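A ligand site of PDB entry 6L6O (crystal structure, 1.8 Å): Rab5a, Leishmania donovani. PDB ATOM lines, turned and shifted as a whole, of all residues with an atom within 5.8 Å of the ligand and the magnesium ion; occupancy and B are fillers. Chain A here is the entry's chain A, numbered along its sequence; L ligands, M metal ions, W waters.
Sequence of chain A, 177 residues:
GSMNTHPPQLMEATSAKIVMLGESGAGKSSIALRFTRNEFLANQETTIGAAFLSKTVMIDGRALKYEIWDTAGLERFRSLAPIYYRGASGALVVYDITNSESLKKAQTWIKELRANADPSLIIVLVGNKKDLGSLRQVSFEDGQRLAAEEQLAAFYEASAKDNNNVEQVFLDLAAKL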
ATOM      1  N   GLY A  22     -17.013  12.089  13.434  1.00  0.00           N
ATOM      2  CA  GLY A  22     -18.476  11.885  13.412  1.00  0.00           C
ATOM      3  C   GLY A  22     -19.180  12.794  14.400  1.00  0.00           C
ATOM      4  O   GLY A  22     -18.580  13.408  15.320  1.00  0.00           O
ATOM      5  N   GLU A  23     -20.470  12.903  14.245  1.00  0.00           N
ATOM      6  CA  GLU A  23     -21.326  13.763  15.085  1.00  0.00           C
ATOM      7  C   GLU A  23     -21.276  13.362  16.537  1.00  0.00           C
ATOM      8  O   GLU A  23     -21.139  12.155  16.843  1.00  0.00           O
ATOM      9  CB  GLU A  23     -22.804  13.645  14.705  1.00  0.00           C
ATOM     10  CG  GLU A  23     -23.094  14.422  13.479  1.00  0.00           C
ATOM     11  CD  GLU A  23     -22.768  15.905  13.559  1.00  0.00           C
ATOM     12  OE1 GLU A  23     -23.647  16.630  14.054  1.00  0.00           O
ATOM     13  OE2 GLU A  23     -21.636  16.330  13.177  1.00  0.00           O
ATOM     14  N   SER A  24     -21.428  14.359  17.394  1.00  0.00           N
ATOM     15  CA  SER A  24     -21.652  14.165  18.846  1.00  0.00           C
ATOM     16  C   SER A  24     -22.667  13.065  19.058  1.00  0.00           C
ATOM     17  O   SER A  24     -23.765  13.125  18.419  1.00  0.00           O
ATOM     18  CB  SER A  24     -22.111  15.464  19.540  1.00  0.00           C
ATOM     19  OG  SER A  24     -21.139  16.520  19.410  1.00  0.00           O
ATOM     20  N   GLY A  25     -22.423  12.153  19.974  1.00  0.00           N
ATOM     21  CA  GLY A  25     -23.402  11.120  20.363  1.00  0.00           C
ATOM     22  C   GLY A  25     -23.385   9.867  19.516  1.00  0.00           C
ATOM     23  O   GLY A  25     -24.114   8.912  19.844  1.00  0.00           O
ATOM     24  N   ALA A  26     -22.595   9.828  18.464  1.00  0.00           N
ATOM     25  CA  ALA A  26     -22.588   8.678  17.543  1.00  0.00           C
ATOM     26  C   ALA A  26     -21.978   7.422  18.211  1.00  0.00           C
ATOM     27  O   ALA A  26     -22.390   6.314  17.841  1.00  0.00           O
ATOM     28  CB  ALA A  26     -21.851   9.046  16.322  1.00  0.00           C
ATOM     29  N   GLY A  27     -21.041   7.614  19.161  1.00  0.00           N
ATOM     30  CA  GLY A  27     -20.318   6.481  19.774  1.00  0.00           C
ATOM     31  C   GLY A  27     -18.820   6.470  19.483  1.00  0.00           C
ATOM     32  O   GLY A  27     -18.233   5.460  19.693  1.00  0.00           O
ATOM     33  N   LYS A  28     -18.212   7.582  19.132  1.00  0.00           N
ATOM     34  CA  LYS A  28     -16.739   7.647  18.864  1.00  0.00           C
ATOM     35  C   LYS A  28     -16.002   7.142  20.104  1.00  0.00           C
ATOM     36  O   LYS A  28     -15.041   6.355  19.965  1.00  0.00           O
ATOM     37  CB  LYS A  28     -16.346   9.083  18.513  1.00  0.00           C
ATOM     38  CG  LYS A  28     -16.917   9.594  17.195  1.00  0.00           C
ATOM     39  CD  LYS A  28     -16.495  11.027  16.821  1.00  0.00           C
ATOM     40  CE  LYS A  28     -16.927  12.040  17.809  1.00  0.00           C
ATOM     41  NZ  LYS A  28     -18.366  12.045  18.053  1.00  0.00           N
ATOM     42  N   SER A  29     -16.264   7.807  21.211  1.00  0.00           N
ATOM     43  CA  SER A  29     -15.530   7.545  22.474  1.00  0.00           C
ATOM     44  C   SER A  29     -15.753   6.070  22.878  1.00  0.00           C
ATOM     45  O   SER A  29     -14.782   5.373  23.288  1.00  0.00           O
ATOM     46  CB  SER A  29     -15.982   8.523  23.511  1.00  0.00           C
ATOM     47  OG  SER A  29     -15.596   9.865  23.164  1.00  0.00           O
ATOM     48  N   SER A  30     -16.961   5.559  22.687  1.00  0.00           N
ATOM     49  CA  SER A  30     -17.325   4.198  23.147  1.00  0.00           C
ATOM     50  C   SER A  30     -16.625   3.190  22.217  1.00  0.00           C
ATOM     51  O   SER A  30     -16.198   2.145  22.689  1.00  0.00           O
ATOM     52  CB  SER A  30     -18.844   4.023  23.201  1.00  0.00           C
ATOM     53  OG  SER A  30     -19.485   4.853  24.146  1.00  0.00           O
ATOM     54  N   ILE A  31     -16.557   3.451  20.914  1.00  0.00           N
ATOM     55  CA  ILE A  31     -15.792   2.538  20.024  1.00  0.00           C
ATOM     56  C   ILE A  31     -14.309   2.510  20.485  1.00  0.00           C
ATOM     57  O   ILE A  31     -13.744   1.421  20.566  1.00  0.00           O
ATOM     58  CB  ILE A  31     -15.990   2.924  18.567  1.00  0.00           C
ATOM     59  CG1 ILE A  31     -17.461   2.648  18.200  1.00  0.00           C
ATOM     60  CG2 ILE A  31     -15.012   2.251  17.627  1.00  0.00           C
ATOM     61  CD1 ILE A  31     -17.795   3.127  16.840  1.00  0.00           C
ATOM     62  N   PHE A  40     -17.170  -0.472  28.368  1.00  0.00           N
ATOM     63  CA  PHE A  40     -18.271   0.358  27.869  1.00  0.00           C
ATOM     64  C   PHE A  40     -18.831   1.184  29.032  1.00  0.00           C
ATOM     65  O   PHE A  40     -19.204   0.601  30.064  1.00  0.00           O
ATOM     66  CB  PHE A  40     -19.339  -0.524  27.228  1.00  0.00           C
ATOM     67  CG  PHE A  40     -20.524   0.288  26.781  1.00  0.00           C
ATOM     68  CD1 PHE A  40     -20.483   0.981  25.567  1.00  0.00           C
ATOM     69  CD2 PHE A  40     -21.664   0.365  27.568  1.00  0.00           C
ATOM     70  CE1 PHE A  40     -21.587   1.706  25.148  1.00  0.00           C
ATOM     71  CE2 PHE A  40     -22.774   1.084  27.134  1.00  0.00           C
ATOM     72  CZ  PHE A  40     -22.726   1.764  25.929  1.00  0.00           C
ATOM     73  N   LEU A  41     -18.912   2.503  28.857  1.00  0.00           N
ATOM     74  CA  LEU A  41     -19.491   3.435  29.854  1.00  0.00           C
ATOM     75  C   LEU A  41     -20.702   4.131  29.221  1.00  0.00           C
ATOM     76  O   LEU A  41     -20.664   4.444  27.953  1.00  0.00           O
ATOM     77  CB  LEU A  41     -18.411   4.432  30.301  1.00  0.00           C
ATOM     78  CG  LEU A  41     -17.083   3.816  30.769  1.00  0.00           C
ATOM     79  CD1 LEU A  41     -16.034   4.898  31.051  1.00  0.00           C
ATOM     80  CD2 LEU A  41     -17.245   2.901  31.985  1.00  0.00           C
ATOM     81  N   ALA A  42     -21.779   4.266  29.993  1.00  0.00           N
ATOM     82  CA  ALA A  42     -23.084   4.881  29.610  1.00  0.00           C
ATOM     83  C   ALA A  42     -23.106   6.384  29.952  1.00  0.00           C
ATOM     84  O   ALA A  42     -22.574   6.758  31.021  1.00  0.00           O
ATOM     85  CB  ALA A  42     -24.187   4.156  30.338  1.00  0.00           C
ATOM     86  N   ASN A  43     -23.794   7.212  29.132  1.00  0.00           N
ATOM     87  CA  ASN A  43     -24.041   8.676  29.323  1.00  0.00           C
ATOM     88  C   ASN A  43     -22.832   9.406  29.930  1.00  0.00           C
ATOM     89  O   ASN A  43     -23.060  10.190  30.874  1.00  0.00           O
ATOM     90  CB  ASN A  43     -25.291   8.957  30.182  1.00  0.00           C
ATOM     91  CG  ASN A  43     -25.696  10.431  30.194  1.00  0.00           C
ATOM     92  N   GLN A  44     -21.609   9.222  29.398  1.00  0.00           N
ATOM     93  CA  GLN A  44     -20.405  10.004  29.852  1.00  0.00           C
ATOM     94  C   GLN A  44     -20.452  11.402  29.236  1.00  0.00           C
ATOM     95  O   GLN A  44     -20.808  11.532  28.056  1.00  0.00           O
ATOM     96  CB  GLN A  44     -19.075   9.332  29.531  1.00  0.00           C
ATOM     97  CG  GLN A  44     -18.939   7.964  30.199  1.00  0.00           C
ATOM     98  CD  GLN A  44     -18.729   8.023  31.699  1.00  0.00           C
ATOM     99  OE1 GLN A  44     -17.681   8.462  32.174  1.00  0.00           O
ATOM    100  NE2 GLN A  44     -19.726   7.548  32.438  1.00  0.00           N
ATOM    101  N   THR A  46     -19.399  14.487  27.325  1.00  0.00           N
ATOM    102  CA  THR A  46     -18.692  14.456  26.001  1.00  0.00           C
ATOM    103  C   THR A  46     -17.230  14.927  26.187  1.00  0.00           C
ATOM    104  O   THR A  46     -16.297  14.434  25.492  1.00  0.00           O
ATOM    105  CB  THR A  46     -19.545  15.271  25.016  1.00  0.00           C
ATOM    106  OG1 THR A  46     -19.088  14.877  23.738  1.00  0.00           O
ATOM    107  CG2 THR A  46     -19.483  16.775  25.213  1.00  0.00           C
ATOM    108  N   ASP A  70      -9.135  10.747  20.018  1.00  0.00           N
ATOM    109  CA  ASP A  70     -10.565  11.004  20.250  1.00  0.00           C
ATOM    110  C   ASP A  70     -10.744  12.523  20.437  1.00  0.00           C
ATOM    111  O   ASP A  70      -9.766  13.287  20.658  1.00  0.00           O
ATOM    112  CB  ASP A  70     -11.126  10.112  21.366  1.00  0.00           C
ATOM    113  CG  ASP A  70     -12.620  10.041  21.425  1.00  0.00           C
ATOM    114  OD1 ASP A  70     -13.280  10.360  20.383  1.00  0.00           O
ATOM    115  OD2 ASP A  70     -13.124   9.811  22.552  1.00  0.00           O
ATOM    116  N   THR A  71     -11.958  13.016  20.286  1.00  0.00           N
ATOM    117  CA  THR A  71     -12.245  14.460  20.081  1.00  0.00           C
ATOM    118  C   THR A  71     -12.308  15.280  21.373  1.00  0.00           C
ATOM    119  O   THR A  71     -12.399  16.535  21.242  1.00  0.00           O
ATOM    120  CB  THR A  71     -13.623  14.631  19.412  1.00  0.00           C
ATOM    121  OG1 THR A  71     -14.646  14.151  20.284  1.00  0.00           O
ATOM    122  CG2 THR A  71     -13.646  13.894  18.110  1.00  0.00           C
ATOM    123  N   ALA A  72     -12.448  14.657  22.547  1.00  0.00           N
ATOM    124  CA  ALA A  72     -12.667  15.358  23.836  1.00  0.00           C
ATOM    125  C   ALA A  72     -13.865  16.288  23.683  1.00  0.00           C
ATOM    126  O   ALA A  72     -13.883  17.350  24.354  1.00  0.00           O
ATOM    127  CB  ALA A  72     -11.438  16.157  24.194  1.00  0.00           C
ATOM    128  N   GLY A  73     -14.875  15.854  22.925  1.00  0.00           N
ATOM    129  CA  GLY A  73     -16.137  16.602  22.862  1.00  0.00           C
ATOM    130  C   GLY A  73     -16.075  17.819  21.971  1.00  0.00           C
ATOM    131  O   GLY A  73     -17.111  18.456  21.851  1.00  0.00           O
ATOM    132  N   GLU A  75     -16.172  18.314  18.858  1.00  0.00           N
ATOM    133  CA  GLU A  75     -17.004  18.263  17.669  1.00  0.00           C
ATOM    134  C   GLU A  75     -18.337  18.914  17.993  1.00  0.00           C
ATOM    135  O   GLU A  75     -19.103  19.070  17.042  1.00  0.00           O
ATOM    136  CB  GLU A  75     -17.195  16.843  17.105  1.00  0.00           C
ATOM    137  CG  GLU A  75     -18.094  15.948  17.916  1.00  0.00           C
ATOM    138  CD  GLU A  75     -17.555  15.294  19.182  1.00  0.00           C
ATOM    139  OE1 GLU A  75     -16.469  15.764  19.702  1.00  0.00           O
ATOM    140  OE2 GLU A  75     -18.202  14.301  19.663  1.00  0.00           O
ATOM    141  N   ASN A 128     -22.786   2.779  14.145  1.00  0.00           N
ATOM    142  CA  ASN A 128     -22.784   2.259  15.535  1.00  0.00           C
ATOM    143  C   ASN A 128     -24.204   2.171  16.125  1.00  0.00           C
ATOM    144  O   ASN A 128     -25.185   2.710  15.567  1.00  0.00           O
ATOM    145  CB  ASN A 128     -21.869   3.119  16.389  1.00  0.00           C
ATOM    146  CG  ASN A 128     -21.624   2.606  17.784  1.00  0.00           C
ATOM    147  OD1 ASN A 128     -21.393   1.389  17.945  1.00  0.00           O
ATOM    148  ND2 ASN A 128     -21.752   3.545  18.743  1.00  0.00           N
ATOM    149  N   LYS A 129     -24.302   1.485  17.231  1.00  0.00           N
ATOM    150  CA  LYS A 129     -25.564   1.199  18.002  1.00  0.00           C
ATOM    151  C   LYS A 129     -26.497   0.298  17.218  1.00  0.00           C
ATOM    152  O   LYS A 129     -27.743   0.403  17.387  1.00  0.00           O
ATOM    153  CB  LYS A 129     -26.309   2.483  18.363  1.00  0.00           C
ATOM    154  CG  LYS A 129     -25.412   3.596  18.895  1.00  0.00           C
ATOM    155  CD  LYS A 129     -26.149   4.711  19.653  1.00  0.00           C
ATOM    156  CE  LYS A 129     -25.227   5.861  19.973  1.00  0.00           C
ATOM    157  NZ  LYS A 129     -25.974   6.993  20.555  1.00  0.00           N
ATOM    158  N   LYS A 130     -25.945  -0.706  16.521  1.00  0.00           N
ATOM    159  CA  LYS A 130     -26.826  -1.676  15.848  1.00  0.00           C
ATOM    160  C   LYS A 130     -27.607  -2.536  16.814  1.00  0.00           C
ATOM    161  O   LYS A 130     -28.593  -3.151  16.345  1.00  0.00           O
ATOM    162  CB  LYS A 130     -26.109  -2.546  14.832  1.00  0.00           C
ATOM    163  CG  LYS A 130     -25.180  -3.578  15.363  1.00  0.00           C
ATOM    164  CD  LYS A 130     -24.698  -4.274  14.053  1.00  0.00           C
ATOM    165  CE  LYS A 130     -24.716  -5.761  14.033  1.00  0.00           C
ATOM    166  NZ  LYS A 130     -23.474  -6.198  14.708  1.00  0.00           N
ATOM    167  N   ASP A 131     -27.284  -2.504  18.083  1.00  0.00           N
ATOM    168  CA  ASP A 131     -28.069  -3.196  19.116  1.00  0.00           C
ATOM    169  C   ASP A 131     -29.438  -2.543  19.274  1.00  0.00           C
ATOM    170  O   ASP A 131     -30.305  -3.207  19.887  1.00  0.00           O
ATOM    171  CB  ASP A 131     -27.391  -3.181  20.459  1.00  0.00           C
ATOM    172  CG  ASP A 131     -26.961  -1.824  20.941  1.00  0.00           C
ATOM    173  OD1 ASP A 131     -25.992  -1.251  20.296  1.00  0.00           O
ATOM    174  OD2 ASP A 131     -27.610  -1.300  21.829  1.00  0.00           O
ATOM    175  N   LEU A 132     -29.589  -1.288  18.866  1.00  0.00           N
ATOM    176  CA  LEU A 132     -30.881  -0.533  19.004  1.00  0.00           C
ATOM    177  C   LEU A 132     -31.753  -0.756  17.750  1.00  0.00           C
ATOM    178  O   LEU A 132     -32.234   0.218  17.149  1.00  0.00           O
ATOM    179  CB  LEU A 132     -30.583   0.937  19.279  1.00  0.00           C
ATOM    180  CG  LEU A 132     -29.832   1.234  20.586  1.00  0.00           C
ATOM    181  CD1 LEU A 132     -29.680   2.734  20.770  1.00  0.00           C
ATOM    182  CD2 LEU A 132     -30.553   0.618  21.809  1.00  0.00           C
ATOM    183  N   ALA A 158     -21.754  -1.759  13.742  1.00  0.00           N
ATOM    184  CA  ALA A 158     -21.134  -2.248  14.986  1.00  0.00           C
ATOM    185  C   ALA A 158     -22.013  -1.883  16.162  1.00  0.00           C
ATOM    186  O   ALA A 158     -22.920  -1.104  16.032  1.00  0.00           O
ATOM    187  CB  ALA A 158     -19.748  -1.707  15.130  1.00  0.00           C
ATOM    188  N   SER A 159     -21.714  -2.442  17.310  1.00  0.00           N
ATOM    189  CA  SER A 159     -22.253  -2.084  18.635  1.00  0.00           C
ATOM    190  C   SER A 159     -21.047  -2.015  19.584  1.00  0.00           C
ATOM    191  O   SER A 159     -20.483  -3.101  19.996  1.00  0.00           O
ATOM    192  CB  SER A 159     -23.333  -2.986  19.178  1.00  0.00           C
ATOM    193  OG  SER A 159     -23.703  -2.583  20.513  1.00  0.00           O
ATOM    194  N   ALA A 160     -20.673  -0.806  19.991  1.00  0.00           N
ATOM    195  CA  ALA A 160     -19.668  -0.616  21.075  1.00  0.00           C
ATOM    196  C   ALA A 160     -20.258  -1.230  22.348  1.00  0.00           C
ATOM    197  O   ALA A 160     -19.496  -1.843  23.146  1.00  0.00           O
ATOM    198  CB  ALA A 160     -19.320   0.821  21.294  1.00  0.00           C
ATOM    199  N   LYS A 161     -21.566  -1.104  22.544  1.00  0.00           N
ATOM    200  CA  LYS A 161     -22.160  -1.637  23.784  1.00  0.00           C
ATOM    201  C   LYS A 161     -22.057  -3.148  23.868  1.00  0.00           C
ATOM    202  O   LYS A 161     -21.719  -3.637  24.918  1.00  0.00           O
ATOM    203  CB  LYS A 161     -23.620  -1.234  23.857  1.00  0.00           C
ATOM    204  CG  LYS A 161     -24.246  -1.706  25.135  1.00  0.00           C
ATOM    205  CD  LYS A 161     -25.633  -1.284  25.186  1.00  0.00           C
ATOM    206  CE  LYS A 161     -26.367  -2.156  26.166  1.00  0.00           C
ATOM    207  NZ  LYS A 161     -27.739  -1.649  26.248  1.00  0.00           N
ATOM    208  N   ASP A 162     -22.397  -3.884  22.824  1.00  0.00           N
ATOM    209  CA  ASP A 162     -22.404  -5.349  22.836  1.00  0.00           C
ATOM    210  C   ASP A 162     -21.053  -5.877  22.365  1.00  0.00           C
ATOM    211  O   ASP A 162     -20.925  -7.107  22.218  1.00  0.00           O
ATOM    212  CB  ASP A 162     -23.504  -5.853  21.903  1.00  0.00           C
ATOM    213  CG  ASP A 162     -24.926  -5.619  22.375  1.00  0.00           C
ATOM    214  OD1 ASP A 162     -25.126  -5.231  23.559  1.00  0.00           O
ATOM    215  OD2 ASP A 162     -25.851  -5.873  21.501  1.00  0.00           O
HETATM  216  P1  LIG L   1     -19.441  10.363  21.063  1.00  0.00           P
HETATM  217  O1  LIG L   1     -20.103  11.656  21.402  1.00  0.00           O
HETATM  218  O2  LIG L   1     -18.002  10.183  21.619  1.00  0.00           O
HETATM  219  O3  LIG L   1     -19.503  10.103  19.561  1.00  0.00           O
HETATM  220  O4  LIG L   1     -20.326   9.183  21.699  1.00  0.00           O
HETATM  221  P2  LIG L   1     -20.217   8.372  23.069  1.00  0.00           P
HETATM  222  O5  LIG L   1     -19.929   9.316  24.142  1.00  0.00           O
HETATM  223  O6  LIG L   1     -19.279   7.258  22.906  1.00  0.00           O
HETATM  224  O7  LIG L   1     -21.646   7.693  23.200  1.00  0.00           O
HETATM  225  C1  LIG L   1     -22.807   8.547  23.139  1.00  0.00           C
HETATM  226  C2  LIG L   1     -23.952   7.814  23.893  1.00  0.00           C
HETATM  227  O8  LIG L   1     -24.348   6.647  23.170  1.00  0.00           O
HETATM  228  C3  LIG L   1     -23.467   7.324  25.274  1.00  0.00           C
HETATM  229  O9  LIG L   1     -24.485   7.419  26.201  1.00  0.00           O
HETATM  230  C4  LIG L   1     -23.104   5.894  25.093  1.00  0.00           C
HETATM  231  O10 LIG L   1     -23.275   5.133  26.272  1.00  0.00           O
HETATM  232  C5  LIG L   1     -24.109   5.496  23.972  1.00  0.00           C
HETATM  233  N1  LIG L   1     -23.593   4.405  23.093  1.00  0.00           N
HETATM  234  C6  LIG L   1     -22.361   4.412  22.508  1.00  0.00           C
HETATM  235  N2  LIG L   1     -22.189   3.364  21.766  1.00  0.00           N
HETATM  236  C7  LIG L   1     -23.369   2.628  21.876  1.00  0.00           C
HETATM  237  C8  LIG L   1     -23.865   1.392  21.393  1.00  0.00           C
HETATM  238  O11 LIG L   1     -23.183   0.701  20.592  1.00  0.00           O
HETATM  239  N3  LIG L   1     -25.111   1.068  21.695  1.00  0.00           N
HETATM  240  C9  LIG L   1     -25.914   1.749  22.593  1.00  0.00           C
HETATM  241  N4  LIG L   1     -27.102   1.312  22.895  1.00  0.00           N
HETATM  242  N5  LIG L   1     -25.533   2.924  23.092  1.00  0.00           N
HETATM  243  C10 LIG L   1     -24.295   3.355  22.740  1.00  0.00           C
HETATM  244 MG    MG M   1     -16.732  11.459  22.592  1.00  0.00          MG
HETATM  245  O   HOH W   1     -21.489  12.471  23.412  1.00  0.00           O
HETATM  246  O   HOH W   2     -15.482  11.683  21.015  1.00  0.00           O
HETATM  247  O   HOH W   3     -24.053  10.590  26.148  1.00  0.00           O
HETATM  248  O   HOH W   4     -27.383   5.297  23.070  1.00  0.00           O
HETATM  249  O   HOH W   5     -28.766   2.154  25.151  1.00  0.00           O
HETATM  250  O   HOH W   6     -15.530  12.685  23.746  1.00  0.00           O
HETATM  251  O   HOH W   7     -17.807  13.104  22.036  1.00  0.00           O
HETATM  252  O   HOH W   8     -17.943  11.234  24.295  1.00  0.00           O
HETATM  253  O   HOH W   9     -20.697   7.257  27.358  1.00  0.00           O
HETATM  254  O   HOH W  10     -18.497   7.989  26.216  1.00  0.00           O
HETATM  255  O   HOH W  11     -21.511  10.856  25.665  1.00  0.00           O
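Merely in contact with the ligand: Glu 23 (3.8 Å), Ser 24 (3.7 Å), Phe 40 (3.4 Å), Ala 42 (3.4 Å), Glu 75 (3.7 Å) and Leu 132 (3.6 Å).
Hydrophobic or aromatic side chains within 4 Å of the ligand: Phe 40, Leu 132 and Ala 160.
Within 4 Å of the ligand: Glu 23, Ser 24, Gly 25, Ala 26, Gly 27, Lys 28, Ser 29, Ser 30, Phe 40, Leu 41, Ala 42, Asn 43, Glu 75, Asn 128, Lys 129, Asp 131, Leu 132, Ser 159, Ala 160 and Lys 161.
The side-chain hydroxyl of Ser 159 sits at hydrogen-bond distance from the backbone NH of Asp 162 (3.0 Å).
O of Ala 158 sits at hydrogen-bond distance from N of Lys 129 (3.2 Å).
OD1 of Asp 131 sits at hydrogen-bond distance from OG of Ser 159, 2.7 Å away.
The side-chain carboxylate (OD2) of Asp 70 sits close to the side-chain hydroxyl (OG) of Ser 29 (2.5 Å).
NZ of Lys 28 lies within hydrogen-bond range of O of Gly 22, 3.1 Å away.
The backbone NH (N) of Lys 161 sits close to the side-chain hydroxyl (OG) of Ser 159, at 3.3 Å.
The side-chain carboxylate (OE1) of Glu 75 lies within hydrogen-bond range of the side-chain hydroxyl (OG1) of Thr 71 (2.5 Å).
O of Ala 158 sits close to OD1 of Asn 128 (3.5 Å).
The backbone NH (N) of Gly 27 lies within hydrogen-bond range of an oxygen (O3) of the ligand (3.0 Å).
O1 of the ligand sits at hydrogen-bond distance from N of Gly 25 (2.8 Å).
The side-chain amino group (NZ) of Lys 28 is in salt-bridge range of an oxygen (O3) of the ligand, at 2.7 Å.
N of Ser 29 lies close to O2 of the ligand.
An oxygen (O3) of the ligand is in hydrogen-bond range of the backbone NH of Ala 26 (3.3 Å).
N of Lys 161 is in hydrogen-bond range of O11 of the ligand (3.1 Å).
The side-chain amino group of Lys 129 lies within hydrogen-bond range of an oxygen (O8) of the ligand, 3.1 Å away.
The backbone NH (N) of Asn 43 is in hydrogen-bond range of an oxygen (O9) of the ligand.
The side-chain hydroxyl (OG) of Ser 30 is in hydrogen-bond range of an oxygen (O6) of the ligand (2.7 Å).
OD1 of Asp 131 lies within hydrogen-bond range of N3 of the ligand (2.8 Å).
N2 of the ligand sits at hydrogen-bond distance from ND2 of Asn 128, at 3.1 Å.
An oxygen (O3) of the ligand sits at hydrogen-bond distance from the backbone NH of Lys 28, at 2.9 Å.
An oxygen (O11) of the ligand lies within hydrogen-bond range of the backbone NH (N) of Ala 160.
The backbone NH of Ser 30 is in hydrogen-bond range of an oxygen (O6) of the ligand, at 2.9 Å.
O of Leu 41 lies within hydrogen-bond range of O10 of the ligand, at 3.2 Å.
An oxygen (O11) of the ligand is in hydrogen-bond range of the side-chain hydroxyl (OG) of Ser 159 (3.3 Å).
Water W7 lies within hydrogen-bond range of the side-chain carboxylate (OE2) of Glu 75 (2.7 Å), the side-chain hydroxyl (OG1) of Thr 46 (2.8 Å) and an oxygen (O1) of the ligand (2.8 Å).
Water W6 bridges the backbone carbonyl oxygen (O) of Thr 46 (2.6 Å) and the backbone NH (N) of Gly 73 (3.3 Å).
Water W2 lies within hydrogen-bond range of OD1 of Asp 70 and OG1 of Thr 71.
Water W1 bridges O1 of the ligand (2.6 Å) and OG1 of Thr 46 (3.4 Å).
Water W11 bridges O of Gln 44 (2.6 Å) and O5 of the ligand (2.7 Å).
Water W4 lies within hydrogen-bond range of N5 of the ligand (3.0 Å) and NZ of Lys 129 (3.3 Å).
Water W2 binds the magnesium ion, at 2.0 Å.
The magnesium ion is bound by OG of Ser 29.
The magnesium ion is bound by water W7 (2.0 Å).
An oxygen (O2) of the ligand is bound to the magnesium ion, 2.0 Å away.
Water W6 binds the magnesium ion, 2.1 Å away.
The magnesium ion is bound by water W8.
The magnesium ion has six donor atoms within binding distance.
Asp 70 touches the magnesium ion (OD2 to MG, 3.97 Å).
Within 4 Å of the magnesium ion: Ser 29 and Asp 70.
The nearest printed residue that does not touch the magnesium ion is Thr 71 (4.1 Å).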
